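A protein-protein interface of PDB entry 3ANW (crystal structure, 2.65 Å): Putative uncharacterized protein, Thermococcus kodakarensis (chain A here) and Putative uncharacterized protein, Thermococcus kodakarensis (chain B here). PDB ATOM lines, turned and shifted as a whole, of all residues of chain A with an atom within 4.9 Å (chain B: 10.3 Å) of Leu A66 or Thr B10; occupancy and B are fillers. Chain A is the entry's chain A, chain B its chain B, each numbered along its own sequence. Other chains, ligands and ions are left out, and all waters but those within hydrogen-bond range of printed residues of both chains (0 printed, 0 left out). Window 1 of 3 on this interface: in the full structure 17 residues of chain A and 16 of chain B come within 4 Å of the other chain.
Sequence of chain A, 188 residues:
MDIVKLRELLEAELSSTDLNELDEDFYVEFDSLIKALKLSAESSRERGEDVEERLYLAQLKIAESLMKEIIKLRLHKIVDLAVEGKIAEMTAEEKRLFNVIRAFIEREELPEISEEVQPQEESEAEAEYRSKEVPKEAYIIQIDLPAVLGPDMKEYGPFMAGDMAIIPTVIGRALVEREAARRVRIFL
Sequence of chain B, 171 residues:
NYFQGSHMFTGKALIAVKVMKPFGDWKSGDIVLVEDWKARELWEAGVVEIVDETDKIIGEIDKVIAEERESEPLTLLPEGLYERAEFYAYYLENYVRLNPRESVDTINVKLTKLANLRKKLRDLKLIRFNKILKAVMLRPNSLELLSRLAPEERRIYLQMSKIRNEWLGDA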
ATOM      1  N   ILE A   3      22.302   1.776  12.115  1.00  0.00           N
ATOM      2  CA  ILE A   3      23.088   1.920  10.904  1.00  0.00           C
ATOM      3  C   ILE A   3      23.195   3.351  10.389  1.00  0.00           C
ATOM      4  O   ILE A   3      24.178   3.706   9.739  1.00  0.00           O
ATOM      5  CB  ILE A   3      22.585   0.982   9.790  1.00  0.00           C
ATOM      6  CG1 ILE A   3      21.100   1.198   9.528  1.00  0.00           C
ATOM      7  CG2 ILE A   3      22.823  -0.462  10.178  1.00  0.00           C
ATOM      8  CD1 ILE A   3      20.536   0.298   8.446  1.00  0.00           C
ATOM      9  N   LEU A   6      26.024   4.983  12.304  1.00  0.00           N
ATOM     10  CA  LEU A   6      27.295   4.449  11.831  1.00  0.00           C
ATOM     11  C   LEU A   6      27.629   5.007  10.440  1.00  0.00           C
ATOM     12  O   LEU A   6      28.792   5.139  10.072  1.00  0.00           O
ATOM     13  CB  LEU A   6      27.277   2.917  11.813  1.00  0.00           C
ATOM     14  CG  LEU A   6      27.200   2.141  13.127  1.00  0.00           C
ATOM     15  CD1 LEU A   6      26.921   0.681  12.847  1.00  0.00           C
ATOM     16  CD2 LEU A   6      28.468   2.294  13.908  1.00  0.00           C
ATOM     17  N   ARG A   7      26.601   5.337   9.673  1.00  0.00           N
ATOM     18  CA  ARG A   7      26.788   5.900   8.352  1.00  0.00           C
ATOM     19  C   ARG A   7      27.317   7.335   8.489  1.00  0.00           C
ATOM     20  O   ARG A   7      28.168   7.768   7.715  1.00  0.00           O
ATOM     21  CB  ARG A   7      25.456   5.882   7.612  1.00  0.00           C
ATOM     22  CG  ARG A   7      25.566   5.634   6.122  1.00  0.00           C
ATOM     23  CD  ARG A   7      24.252   5.195   5.550  1.00  0.00           C
ATOM     24  NE  ARG A   7      23.203   6.138   5.897  1.00  0.00           N
ATOM     25  CZ  ARG A   7      21.955   5.801   6.181  1.00  0.00           C
ATOM     26  NH1 ARG A   7      21.580   4.534   6.146  1.00  0.00           N
ATOM     27  NH2 ARG A   7      21.103   6.732   6.567  1.00  0.00           N
ATOM     28  N   LEU A  10      31.007   7.371   9.754  1.00  0.00           N
ATOM     29  CA  LEU A  10      31.938   6.931   8.725  1.00  0.00           C
ATOM     30  C   LEU A  10      32.218   8.084   7.793  1.00  0.00           C
ATOM     31  O   LEU A  10      33.328   8.259   7.311  1.00  0.00           O
ATOM     32  CB  LEU A  10      31.383   5.742   7.943  1.00  0.00           C
ATOM     33  CG  LEU A  10      32.227   5.225   6.774  1.00  0.00           C
ATOM     34  CD1 LEU A  10      33.609   4.815   7.250  1.00  0.00           C
ATOM     35  CD2 LEU A  10      31.516   4.090   6.076  1.00  0.00           C
ATOM     36  N   ILE A  62      25.255  -4.758   7.189  1.00  0.00           N
ATOM     37  CA  ILE A  62      25.570  -3.353   6.969  1.00  0.00           C
ATOM     38  C   ILE A  62      26.281  -2.769   8.196  1.00  0.00           C
ATOM     39  O   ILE A  62      27.140  -1.908   8.075  1.00  0.00           O
ATOM     40  CB  ILE A  62      24.285  -2.536   6.680  1.00  0.00           C
ATOM     41  CG1 ILE A  62      23.644  -3.013   5.386  1.00  0.00           C
ATOM     42  CG2 ILE A  62      24.588  -1.042   6.599  1.00  0.00           C
ATOM     43  CD1 ILE A  62      22.352  -2.346   5.111  1.00  0.00           C
ATOM     44  N   ALA A  63      25.921  -3.260   9.373  1.00  0.00           N
ATOM     45  CA  ALA A  63      26.503  -2.793  10.615  1.00  0.00           C
ATOM     46  C   ALA A  63      27.948  -3.243  10.708  1.00  0.00           C
ATOM     47  O   ALA A  63      28.833  -2.455  11.032  1.00  0.00           O
ATOM     48  CB  ALA A  63      25.708  -3.318  11.787  1.00  0.00           C
ATOM     49  N   GLU A  64      28.178  -4.517  10.413  1.00  0.00           N
ATOM     50  CA  GLU A  64      29.514  -5.087  10.441  1.00  0.00           C
ATOM     51  C   GLU A  64      30.393  -4.437   9.382  1.00  0.00           C
ATOM     52  O   GLU A  64      31.580  -4.249   9.587  1.00  0.00           O
ATOM     53  CB  GLU A  64      29.462  -6.605  10.246  1.00  0.00           C
ATOM     54  CG  GLU A  64      28.879  -7.357  11.420  1.00  0.00           C
ATOM     55  CD  GLU A  64      29.731  -7.277  12.699  1.00  0.00           C
ATOM     56  OE1 GLU A  64      30.682  -6.460  12.761  1.00  0.00           O
ATOM     57  OE2 GLU A  64      29.452  -8.044  13.657  1.00  0.00           O
ATOM     58  N   SER A  65      29.795  -4.080   8.260  1.00  0.00           N
ATOM     59  CA  SER A  65      30.510  -3.433   7.186  1.00  0.00           C
ATOM     60  C   SER A  65      30.873  -1.987   7.561  1.00  0.00           C
ATOM     61  O   SER A  65      32.017  -1.567   7.391  1.00  0.00           O
ATOM     62  CB  SER A  65      29.664  -3.470   5.911  1.00  0.00           C
ATOM     63  OG  SER A  65      30.327  -2.859   4.818  1.00  0.00           O
ATOM     64  N   LEU A  66      29.910  -1.229   8.074  1.00  0.00           N
ATOM     65  CA  LEU A  66      30.176   0.150   8.452  1.00  0.00           C
ATOM     66  C   LEU A  66      31.245   0.174   9.524  1.00  0.00           C
ATOM     67  O   LEU A  66      32.196   0.935   9.435  1.00  0.00           O
ATOM     68  CB  LEU A  66      28.904   0.865   8.936  1.00  0.00           C
ATOM     69  CG  LEU A  66      27.814   1.114   7.883  1.00  0.00           C
ATOM     70  CD1 LEU A  66      26.621   1.810   8.483  1.00  0.00           C
ATOM     71  CD2 LEU A  66      28.352   1.920   6.735  1.00  0.00           C
ATOM     72  N   MET A  67      31.118  -0.704  10.507  1.00  0.00           N
ATOM     73  CA  MET A  67      32.083  -0.777  11.589  1.00  0.00           C
ATOM     74  C   MET A  67      33.498  -1.074  11.083  1.00  0.00           C
ATOM     75  O   MET A  67      34.465  -0.460  11.525  1.00  0.00           O
ATOM     76  CB  MET A  67      31.655  -1.848  12.587  1.00  0.00           C
ATOM     77  CG  MET A  67      32.575  -1.970  13.765  1.00  0.00           C
ATOM     78  SD  MET A  67      32.705  -0.385  14.543  1.00  0.00           S
ATOM     79  CE  MET A  67      32.440  -0.786  16.192  1.00  0.00           C
ATOM     80  N   LYS A  68      33.603  -2.019  10.155  1.00  0.00           N
ATOM     81  CA  LYS A  68      34.877  -2.417   9.580  1.00  0.00           C
ATOM     82  C   LYS A  68      35.587  -1.212   8.950  1.00  0.00           C
ATOM     83  O   LYS A  68      36.774  -0.984   9.171  1.00  0.00           O
ATOM     84  CB  LYS A  68      34.642  -3.502   8.531  1.00  0.00           C
ATOM     85  CG  LYS A  68      35.872  -4.323   8.150  1.00  0.00           C
ATOM     86  CD  LYS A  68      35.557  -5.210   6.959  1.00  0.00           C
ATOM     87  CE  LYS A  68      36.686  -6.154   6.621  1.00  0.00           C
ATOM     88  NZ  LYS A  68      36.317  -7.077   5.506  1.00  0.00           N
ATOM     89  N   GLU A  69      34.850  -0.432   8.174  1.00  0.00           N
ATOM     90  CA  GLU A  69      35.421   0.736   7.542  1.00  0.00           C
ATOM     91  C   GLU A  69      35.802   1.798   8.537  1.00  0.00           C
ATOM     92  O   GLU A  69      36.804   2.467   8.349  1.00  0.00           O
ATOM     93  CB  GLU A  69      34.469   1.316   6.520  1.00  0.00           C
ATOM     94  CG  GLU A  69      34.621   0.714   5.154  1.00  0.00           C
ATOM     95  CD  GLU A  69      33.812   1.446   4.123  1.00  0.00           C
ATOM     96  OE1 GLU A  69      32.603   1.145   4.031  1.00  0.00           O
ATOM     97  OE2 GLU A  69      34.378   2.330   3.425  1.00  0.00           O
ATOM     98  N   ILE A  70      35.008   1.957   9.591  1.00  0.00           N
ATOM     99  CA  ILE A  70      35.292   2.959  10.620  1.00  0.00           C
ATOM    100  C   ILE A  70      36.540   2.631  11.442  1.00  0.00           C
ATOM    101  O   ILE A  70      37.362   3.499  11.693  1.00  0.00           O
ATOM    102  CB  ILE A  70      34.094   3.151  11.596  1.00  0.00           C
ATOM    103  CG1 ILE A  70      32.876   3.678  10.849  1.00  0.00           C
ATOM    104  CG2 ILE A  70      34.454   4.133  12.691  1.00  0.00           C
ATOM    105  CD1 ILE A  70      31.644   3.741  11.685  1.00  0.00           C
ATOM    106  N   SER B   6      29.329  -8.613  -3.322  1.00  0.00           N
ATOM    107  CA  SER B   6      29.288  -7.531  -4.325  1.00  0.00           C
ATOM    108  C   SER B   6      29.194  -6.152  -3.640  1.00  0.00           C
ATOM    109  O   SER B   6      29.476  -6.032  -2.442  1.00  0.00           O
ATOM    110  CB  SER B   6      28.120  -7.739  -5.300  1.00  0.00           C
ATOM    111  N   HIS B   7      28.829  -5.114  -4.393  1.00  0.00           N
ATOM    112  CA  HIS B   7      28.698  -3.761  -3.834  1.00  0.00           C
ATOM    113  C   HIS B   7      27.695  -3.755  -2.693  1.00  0.00           C
ATOM    114  O   HIS B   7      26.641  -4.391  -2.784  1.00  0.00           O
ATOM    115  CB  HIS B   7      28.244  -2.766  -4.907  1.00  0.00           C
ATOM    116  CG  HIS B   7      27.979  -1.384  -4.383  1.00  0.00           C
ATOM    117  ND1 HIS B   7      28.980  -0.457  -4.179  1.00  0.00           N
ATOM    118  CD2 HIS B   7      26.827  -0.780  -4.002  1.00  0.00           C
ATOM    119  CE1 HIS B   7      28.458   0.653  -3.688  1.00  0.00           C
ATOM    120  NE2 HIS B   7      27.154   0.483  -3.572  1.00  0.00           N
ATOM    121  N   MET B   8      28.004  -3.018  -1.630  1.00  0.00           N
ATOM    122  CA  MET B   8      27.098  -2.982  -0.493  1.00  0.00           C
ATOM    123  C   MET B   8      26.385  -1.668  -0.244  1.00  0.00           C
ATOM    124  O   MET B   8      27.025  -0.634  -0.036  1.00  0.00           O
ATOM    125  CB  MET B   8      27.814  -3.409   0.780  1.00  0.00           C
ATOM    126  CG  MET B   8      26.862  -3.621   1.941  1.00  0.00           C
ATOM    127  SD  MET B   8      27.582  -4.644   3.186  1.00  0.00           S
ATOM    128  CE  MET B   8      27.909  -6.132   2.223  1.00  0.00           C
ATOM    129  N   PHE B   9      25.056  -1.735  -0.190  1.00  0.00           N
ATOM    130  CA  PHE B   9      24.232  -0.560   0.051  1.00  0.00           C
ATOM    131  C   PHE B   9      24.038  -0.380   1.543  1.00  0.00           C
ATOM    132  O   PHE B   9      23.658  -1.312   2.252  1.00  0.00           O
ATOM    133  CB  PHE B   9      22.898  -0.704  -0.676  1.00  0.00           C
ATOM    134  CG  PHE B   9      23.042  -0.888  -2.149  1.00  0.00           C
ATOM    135  CD1 PHE B   9      23.029  -2.153  -2.706  1.00  0.00           C
ATOM    136  CD2 PHE B   9      23.241   0.204  -2.980  1.00  0.00           C
ATOM    137  CE1 PHE B   9      23.216  -2.331  -4.076  1.00  0.00           C
ATOM    138  CE2 PHE B   9      23.429   0.034  -4.354  1.00  0.00           C
ATOM    139  CZ  PHE B   9      23.416  -1.234  -4.900  1.00  0.00           C
ATOM    140  N   THR B  10      24.338   0.816   2.028  1.00  0.00           N
ATOM    141  CA  THR B  10      24.218   1.096   3.446  1.00  0.00           C
ATOM    142  C   THR B  10      23.093   2.049   3.789  1.00  0.00           C
ATOM    143  O   THR B  10      22.876   2.359   4.951  1.00  0.00           O
ATOM    144  CB  THR B  10      25.540   1.611   4.011  1.00  0.00           C
ATOM    145  OG1 THR B  10      25.987   2.734   3.249  1.00  0.00           O
ATOM    146  CG2 THR B  10      26.582   0.543   3.914  1.00  0.00           C
ATOM    147  N   GLY B  11      22.351   2.477   2.781  1.00  0.00           N
ATOM    148  CA  GLY B  11      21.245   3.381   3.024  1.00  0.00           C
ATOM    149  C   GLY B  11      21.530   4.835   2.729  1.00  0.00           C
ATOM    150  O   GLY B  11      20.827   5.714   3.192  1.00  0.00           O
ATOM    151  N   LYS B  12      22.568   5.094   1.955  1.00  0.00           N
ATOM    152  CA  LYS B  12      22.922   6.457   1.614  1.00  0.00           C
ATOM    153  C   LYS B  12      22.002   7.051   0.561  1.00  0.00           C
ATOM    154  O   LYS B  12      21.929   8.260   0.426  1.00  0.00           O
ATOM    155  CB  LYS B  12      24.380   6.521   1.161  1.00  0.00           C
ATOM    156  CG  LYS B  12      25.353   6.174   2.283  1.00  0.00           C
ATOM    157  CD  LYS B  12      26.785   6.569   1.981  1.00  0.00           C
ATOM    158  CE  LYS B  12      27.394   5.639   0.970  1.00  0.00           C
ATOM    159  NZ  LYS B  12      28.834   5.915   0.814  1.00  0.00           N
ATOM    160  N   ALA B  13      21.285   6.200  -0.164  1.00  0.00           N
ATOM    161  CA  ALA B  13      20.371   6.657  -1.200  1.00  0.00           C
ATOM    162  C   ALA B  13      18.942   6.190  -0.945  1.00  0.00           C
ATOM    163  O   ALA B  13      18.720   5.151  -0.328  1.00  0.00           O
ATOM    164  CB  ALA B  13      20.841   6.180  -2.556  1.00  0.00           C
ATOM    165  N   LEU B  14      17.982   7.004  -1.378  1.00  0.00           N
ATOM    166  CA  LEU B  14      16.568   6.694  -1.239  1.00  0.00           C
ATOM    167  C   LEU B  14      16.066   6.275  -2.605  1.00  0.00           C
ATOM    168  O   LEU B  14      16.301   6.954  -3.608  1.00  0.00           O
ATOM    169  CB  LEU B  14      15.775   7.897  -0.725  1.00  0.00           C
ATOM    170  CG  LEU B  14      16.022   8.312   0.727  1.00  0.00           C
ATOM    171  CD1 LEU B  14      15.262   9.577   1.055  1.00  0.00           C
ATOM    172  CD2 LEU B  14      15.629   7.193   1.680  1.00  0.00           C
ATOM    173  N   ILE B  15      15.420   5.115  -2.628  1.00  0.00           N
ATOM    174  CA  ILE B  15      14.878   4.529  -3.844  1.00  0.00           C
ATOM    175  C   ILE B  15      13.353   4.451  -3.818  1.00  0.00           C
ATOM    176  O   ILE B  15      12.766   3.967  -2.851  1.00  0.00           O
ATOM    177  CB  ILE B  15      15.420   3.106  -4.038  1.00  0.00           C
ATOM    178  CG1 ILE B  15      16.947   3.104  -3.997  1.00  0.00           C
ATOM    179  CG2 ILE B  15      14.887   2.500  -5.323  1.00  0.00           C
ATOM    180  CD1 ILE B  15      17.611   3.938  -5.055  1.00  0.00           C
ATOM    181  N   VAL B  34      12.399   4.286   0.027  1.00  0.00           N
ATOM    182  CA  VAL B  34      13.127   3.498   1.022  1.00  0.00           C
ATOM    183  C   VAL B  34      14.630   3.628   0.809  1.00  0.00           C
ATOM    184  O   VAL B  34      15.074   4.092  -0.236  1.00  0.00           O
ATOM    185  CB  VAL B  34      12.779   1.972   0.929  1.00  0.00           C
ATOM    186  CG1 VAL B  34      11.493   1.663   1.654  1.00  0.00           C
ATOM    187  CG2 VAL B  34      12.694   1.541  -0.507  1.00  0.00           C
ATOM    188  N   GLU B  35      15.411   3.189   1.791  1.00  0.00           N
ATOM    189  CA  GLU B  35      16.858   3.234   1.672  1.00  0.00           C
ATOM    190  C   GLU B  35      17.285   2.142   0.710  1.00  0.00           C
ATOM    191  O   GLU B  35      16.774   1.040   0.786  1.00  0.00           O
ATOM    192  CB  GLU B  35      17.492   3.025   3.032  1.00  0.00           C
ATOM    193  CG  GLU B  35      16.999   4.018   4.051  1.00  0.00           C
ATOM    194  CD  GLU B  35      17.945   4.209   5.202  1.00  0.00           C
ATOM    195  OE1 GLU B  35      18.734   3.302   5.495  1.00  0.00           O
ATOM    196  OE2 GLU B  35      17.898   5.281   5.821  1.00  0.00           O
ATOM    197  N   ASP B  36      18.197   2.466  -0.206  1.00  0.00           N
ATOM    198  CA  ASP B  36      18.702   1.531  -1.219  1.00  0.00           C
ATOM    199  C   ASP B  36      18.828   0.059  -0.817  1.00  0.00           C
ATOM    200  O   ASP B  36      18.456  -0.838  -1.579  1.00  0.00           O
ATOM    201  CB  ASP B  36      20.042   2.021  -1.777  1.00  0.00           C
ATOM    202  CG  ASP B  36      21.042   2.414  -0.689  1.00  0.00           C
ATOM    203  OD1 ASP B  36      21.070   1.782   0.380  1.00  0.00           O
ATOM    204  OD2 ASP B  36      21.816   3.364  -0.906  1.00  0.00           O
ATOM    205  N   TRP B  37      19.343  -0.181   0.382  1.00  0.00           N
ATOM    206  CA  TRP B  37      19.527  -1.527   0.888  1.00  0.00           C
ATOM    207  C   TRP B  37      18.193  -2.206   1.180  1.00  0.00           C
ATOM    208  O   TRP B  37      18.059  -3.419   1.024  1.00  0.00           O
ATOM    209  CB  TRP B  37      20.388  -1.492   2.151  1.00  0.00           C
ATOM    210  CG  TRP B  37      19.694  -0.951   3.358  1.00  0.00           C
ATOM    211  CD1 TRP B  37      19.746   0.317   3.821  1.00  0.00           C
ATOM    212  CD2 TRP B  37      18.851  -1.676   4.264  1.00  0.00           C
ATOM    213  NE1 TRP B  37      18.992   0.439   4.962  1.00  0.00           N
ATOM    214  CE2 TRP B  37      18.429  -0.772   5.252  1.00  0.00           C
ATOM    215  CE3 TRP B  37      18.413  -3.001   4.332  1.00  0.00           C
ATOM    216  CZ2 TRP B  37      17.590  -1.145   6.298  1.00  0.00           C
ATOM    217  CZ3 TRP B  37      17.579  -3.376   5.372  1.00  0.00           C
ATOM    218  CH2 TRP B  37      17.175  -2.449   6.343  1.00  0.00           C
ATOM    219  N   LYS B  38      17.228  -1.419   1.655  1.00  0.00           N
ATOM    220  CA  LYS B  38      15.894  -1.917   1.984  1.00  0.00           C
ATOM    221  C   LYS B  38      15.117  -2.093   0.692  1.00  0.00           C
ATOM    222  O   LYS B  38      14.165  -2.851   0.632  1.00  0.00           O
ATOM    223  CB  LYS B  38      15.179  -0.948   2.937  1.00  0.00           C
ATOM    224  CG  LYS B  38      13.961  -1.525   3.631  1.00  0.00           C
ATOM    225  CD  LYS B  38      13.640  -0.762   4.901  1.00  0.00           C
ATOM    226  CE  LYS B  38      12.509  -1.418   5.676  1.00  0.00           C
ATOM    227  NZ  LYS B  38      12.448  -0.963   7.093  1.00  0.00           N
ATOM    228  N   ALA B  39      15.555  -1.397  -0.347  1.00  0.00           N
ATOM    229  CA  ALA B  39      14.930  -1.487  -1.652  1.00  0.00           C
ATOM    230  C   ALA B  39      15.322  -2.796  -2.304  1.00  0.00           C
ATOM    231  O   ALA B  39      14.477  -3.469  -2.878  1.00  0.00           O
ATOM    232  CB  ALA B  39      15.358  -0.326  -2.526  1.00  0.00           C
ATOM    233  N   ARG B  40      16.598  -3.166  -2.216  1.00  0.00           N
ATOM    234  CA  ARG B  40      17.028  -4.418  -2.826  1.00  0.00           C
ATOM    235  C   ARG B  40      16.499  -5.642  -2.069  1.00  0.00           C
ATOM    236  O   ARG B  40      16.128  -6.635  -2.691  1.00  0.00           O
ATOM    237  CB  ARG B  40      18.558  -4.478  -3.018  1.00  0.00           C
ATOM    238  CG  ARG B  40      19.367  -5.001  -1.849  1.00  0.00           C
ATOM    239  CD  ARG B  40      20.225  -6.189  -2.264  1.00  0.00           C
ATOM    240  NE  ARG B  40      21.239  -5.821  -3.250  1.00  0.00           N
ATOM    241  CZ  ARG B  40      22.470  -6.333  -3.301  1.00  0.00           C
ATOM    242  NH1 ARG B  40      22.858  -7.250  -2.424  1.00  0.00           N
ATOM    243  NH2 ARG B  40      23.332  -5.905  -4.219  1.00  0.00           N
ATOM    244  N   GLU B  41      16.402  -5.542  -0.745  1.00  0.00           N
ATOM    245  CA  GLU B  41      15.906  -6.660   0.058  1.00  0.00           C
ATOM    246  C   GLU B  41      14.422  -6.940  -0.166  1.00  0.00           C
ATOM    247  O   GLU B  41      14.046  -8.090  -0.382  1.00  0.00           O
ATOM    248  CB  GLU B  41      16.186  -6.473   1.559  1.00  0.00           C
ATOM    249  CG  GLU B  41      17.662  -6.602   1.968  1.00  0.00           C
ATOM    250  CD  GLU B  41      18.296  -7.949   1.625  1.00  0.00           C
ATOM    251  OE1 GLU B  41      18.940  -8.065   0.561  1.00  0.00           O
ATOM    252  OE2 GLU B  41      18.181  -8.885   2.438  1.00  0.00           O
ATOM    253  N   GLU B  83      25.797   6.836  -5.137  1.00  0.00           N
ATOM    254  CA  GLU B  83      25.047   5.697  -4.596  1.00  0.00           C
ATOM    255  C   GLU B  83      23.780   5.318  -5.369  1.00  0.00           C
ATOM    256  O   GLU B  83      23.455   4.132  -5.470  1.00  0.00           O
ATOM    257  CB  GLU B  83      24.704   5.902  -3.117  1.00  0.00           C
ATOM    258  CG  GLU B  83      25.820   5.531  -2.132  1.00  0.00           C
ATOM    259  CD  GLU B  83      26.101   4.016  -2.045  1.00  0.00           C
ATOM    260  OE1 GLU B  83      26.790   3.493  -2.951  1.00  0.00           O
ATOM    261  OE2 GLU B  83      25.648   3.356  -1.068  1.00  0.00           O
ATOM    262  N   ARG B  84      23.066   6.318  -5.895  1.00  0.00           N
ATOM    263  CA  ARG B  84      21.834   6.092  -6.661  1.00  0.00           C
ATOM    264  C   ARG B  84      22.132   5.507  -8.035  1.00  0.00           C
ATOM    265  O   ARG B  84      21.316   4.803  -8.604  1.00  0.00           O
ATOM    266  CB  ARG B  84      21.008   7.382  -6.800  1.00  0.00           C
ATOM    267  CG  ARG B  84      20.651   8.053  -5.468  1.00  0.00           C
ATOM    268  CD  ARG B  84      19.589   9.146  -5.591  1.00  0.00           C
ATOM    269  NE  ARG B  84      19.611   9.819  -6.887  1.00  0.00           N
ATOM    270  CZ  ARG B  84      20.213  10.974  -7.142  1.00  0.00           C
ATOM    271  NH1 ARG B  84      20.863  11.623  -6.197  1.00  0.00           N
ATOM    272  NH2 ARG B  84      20.168  11.478  -8.358  1.00  0.00           N
ATOM    273  N   GLU B  86      24.672   3.463  -8.532  1.00  0.00           N
ATOM    274  CA  GLU B  86      25.032   2.094  -8.194  1.00  0.00           C
ATOM    275  C   GLU B  86      23.807   1.207  -8.098  1.00  0.00           C
ATOM    276  O   GLU B  86      23.814   0.079  -8.597  1.00  0.00           O
ATOM    277  CB  GLU B  86      25.805   2.038  -6.866  1.00  0.00           C
ATOM    278  CG  GLU B  86      27.318   2.330  -6.960  1.00  0.00           C
ATOM    279  CD  GLU B  86      28.151   1.225  -7.647  1.00  0.00           C
ATOM    280  OE1 GLU B  86      27.597   0.237  -8.196  1.00  0.00           O
ATOM    281  OE2 GLU B  86      29.393   1.359  -7.631  1.00  0.00           O
ATOM    282  N   PHE B  87      22.750   1.725  -7.472  1.00  0.00           N
ATOM    283  CA  PHE B  87      21.526   0.957  -7.323  1.00  0.00           C
ATOM    284  C   PHE B  87      20.804   0.582  -8.623  1.00  0.00           C
ATOM    285  O   PHE B  87      20.333  -0.543  -8.774  1.00  0.00           O
ATOM    286  CB  PHE B  87      20.546   1.632  -6.382  1.00  0.00           C
ATOM    287  CG  PHE B  87      19.341   0.791  -6.110  1.00  0.00           C
ATOM    288  CD1 PHE B  87      19.367  -0.170  -5.113  1.00  0.00           C
ATOM    289  CD2 PHE B  87      18.208   0.892  -6.913  1.00  0.00           C
ATOM    290  CE1 PHE B  87      18.291  -1.013  -4.923  1.00  0.00           C
ATOM    291  CE2 PHE B  87      17.137   0.052  -6.728  1.00  0.00           C
ATOM    292  CZ  PHE B  87      17.175  -0.902  -5.734  1.00  0.00           C
ATOM    293  N   GLU B 152      34.068  10.027   0.317  1.00  0.00           N
ATOM    294  CA  GLU B 152      35.141   9.125  -0.105  1.00  0.00           C
ATOM    295  C   GLU B 152      36.229   9.881  -0.878  1.00  0.00           C
ATOM    296  O   GLU B 152      37.396   9.521  -0.791  1.00  0.00           O
ATOM    297  CB  GLU B 152      34.597   7.971  -0.960  1.00  0.00           C
ATOM    298  CG  GLU B 152      33.263   7.368  -0.490  1.00  0.00           C
ATOM    299  CD  GLU B 152      32.024   8.122  -1.012  1.00  0.00           C
ATOM    300  OE1 GLU B 152      30.943   7.508  -1.130  1.00  0.00           O
ATOM    301  OE2 GLU B 152      32.117   9.324  -1.319  1.00  0.00           O
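The backbone carbonyl oxygen (O) of Thr B10 lies within hydrogen-bond range of the guanidinium group (NH1) of Arg A7 (2.8 Å). NH1 of Arg A7 lies close to O of Gly B11, 3.3 Å away. The side-chain carboxylate (OE1) of Glu B35 is in salt-bridge range of the guanidinium group (NH1) of Arg A7 (3.2 Å). The side-chain hydroxyl of Ser A65 lies close to the side-chain sulfur of Met B8 (3.7 Å).
The side-chain carboxylate (OD1) of Asp B36 is in hydrogen-bond range of the backbone NH (N) of Gly B11. N of Lys B12 sits at hydrogen-bond distance from OD2 of Asp B36 (3.4 Å). The side-chain amino group (NZ) of Lys B12 lies within salt-bridge range of the side-chain carboxylate (OE1) of Glu B152. NE1 of Trp B37 lies within hydrogen-bond range of OE1 of Glu B35.
Among the printed residues, merely in contact across the chains: Ile A62 with Phe B9 (3.3 Å), Ile A62 with Trp B37 (3.5 Å), Arg A7 with Lys B12 (3.6 Å), Leu A66 with Thr B10 (3.6 Å), Ile A62 with Thr B10 (3.7 Å) and Ile A3 with Trp B37 (3.8 Å).
Of chain B, only Thr B10 (3.6 Å) comes within 4 Å of Leu A66. Of chain A, only Arg A7, Ile A62 and Leu A66 come within 4 Å of Thr B10. Ile A3 touches one residue of chain B. No residue of chain B comes within 4 Å of Leu A6. Arg A7 touches four residues of chain B. Ala A63 touches none of the printed residues of chain B. No residue of chain B comes within 4 Å of Ile A70. Printed residues of chain A within 4 Å of Gly B11: Arg A7 (3.2 Å). Of the printed residues of chain A, Met B8 touches Ser A65. Of the printed residues of chain A, Phe B9 touches Ile A62 (3.3 Å). The nearest residue of chain A that does not touch Thr B10 is Ile A3 (4.7 Å). The nearest printed residue of chain A that does not touch Phe B9 is Arg A7 (6.9 Å).
Along chain A the printed residues that touch a printed residue of chain B span positions 3 to 66. Among the printed residues, 10 pairs touch across the chains.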
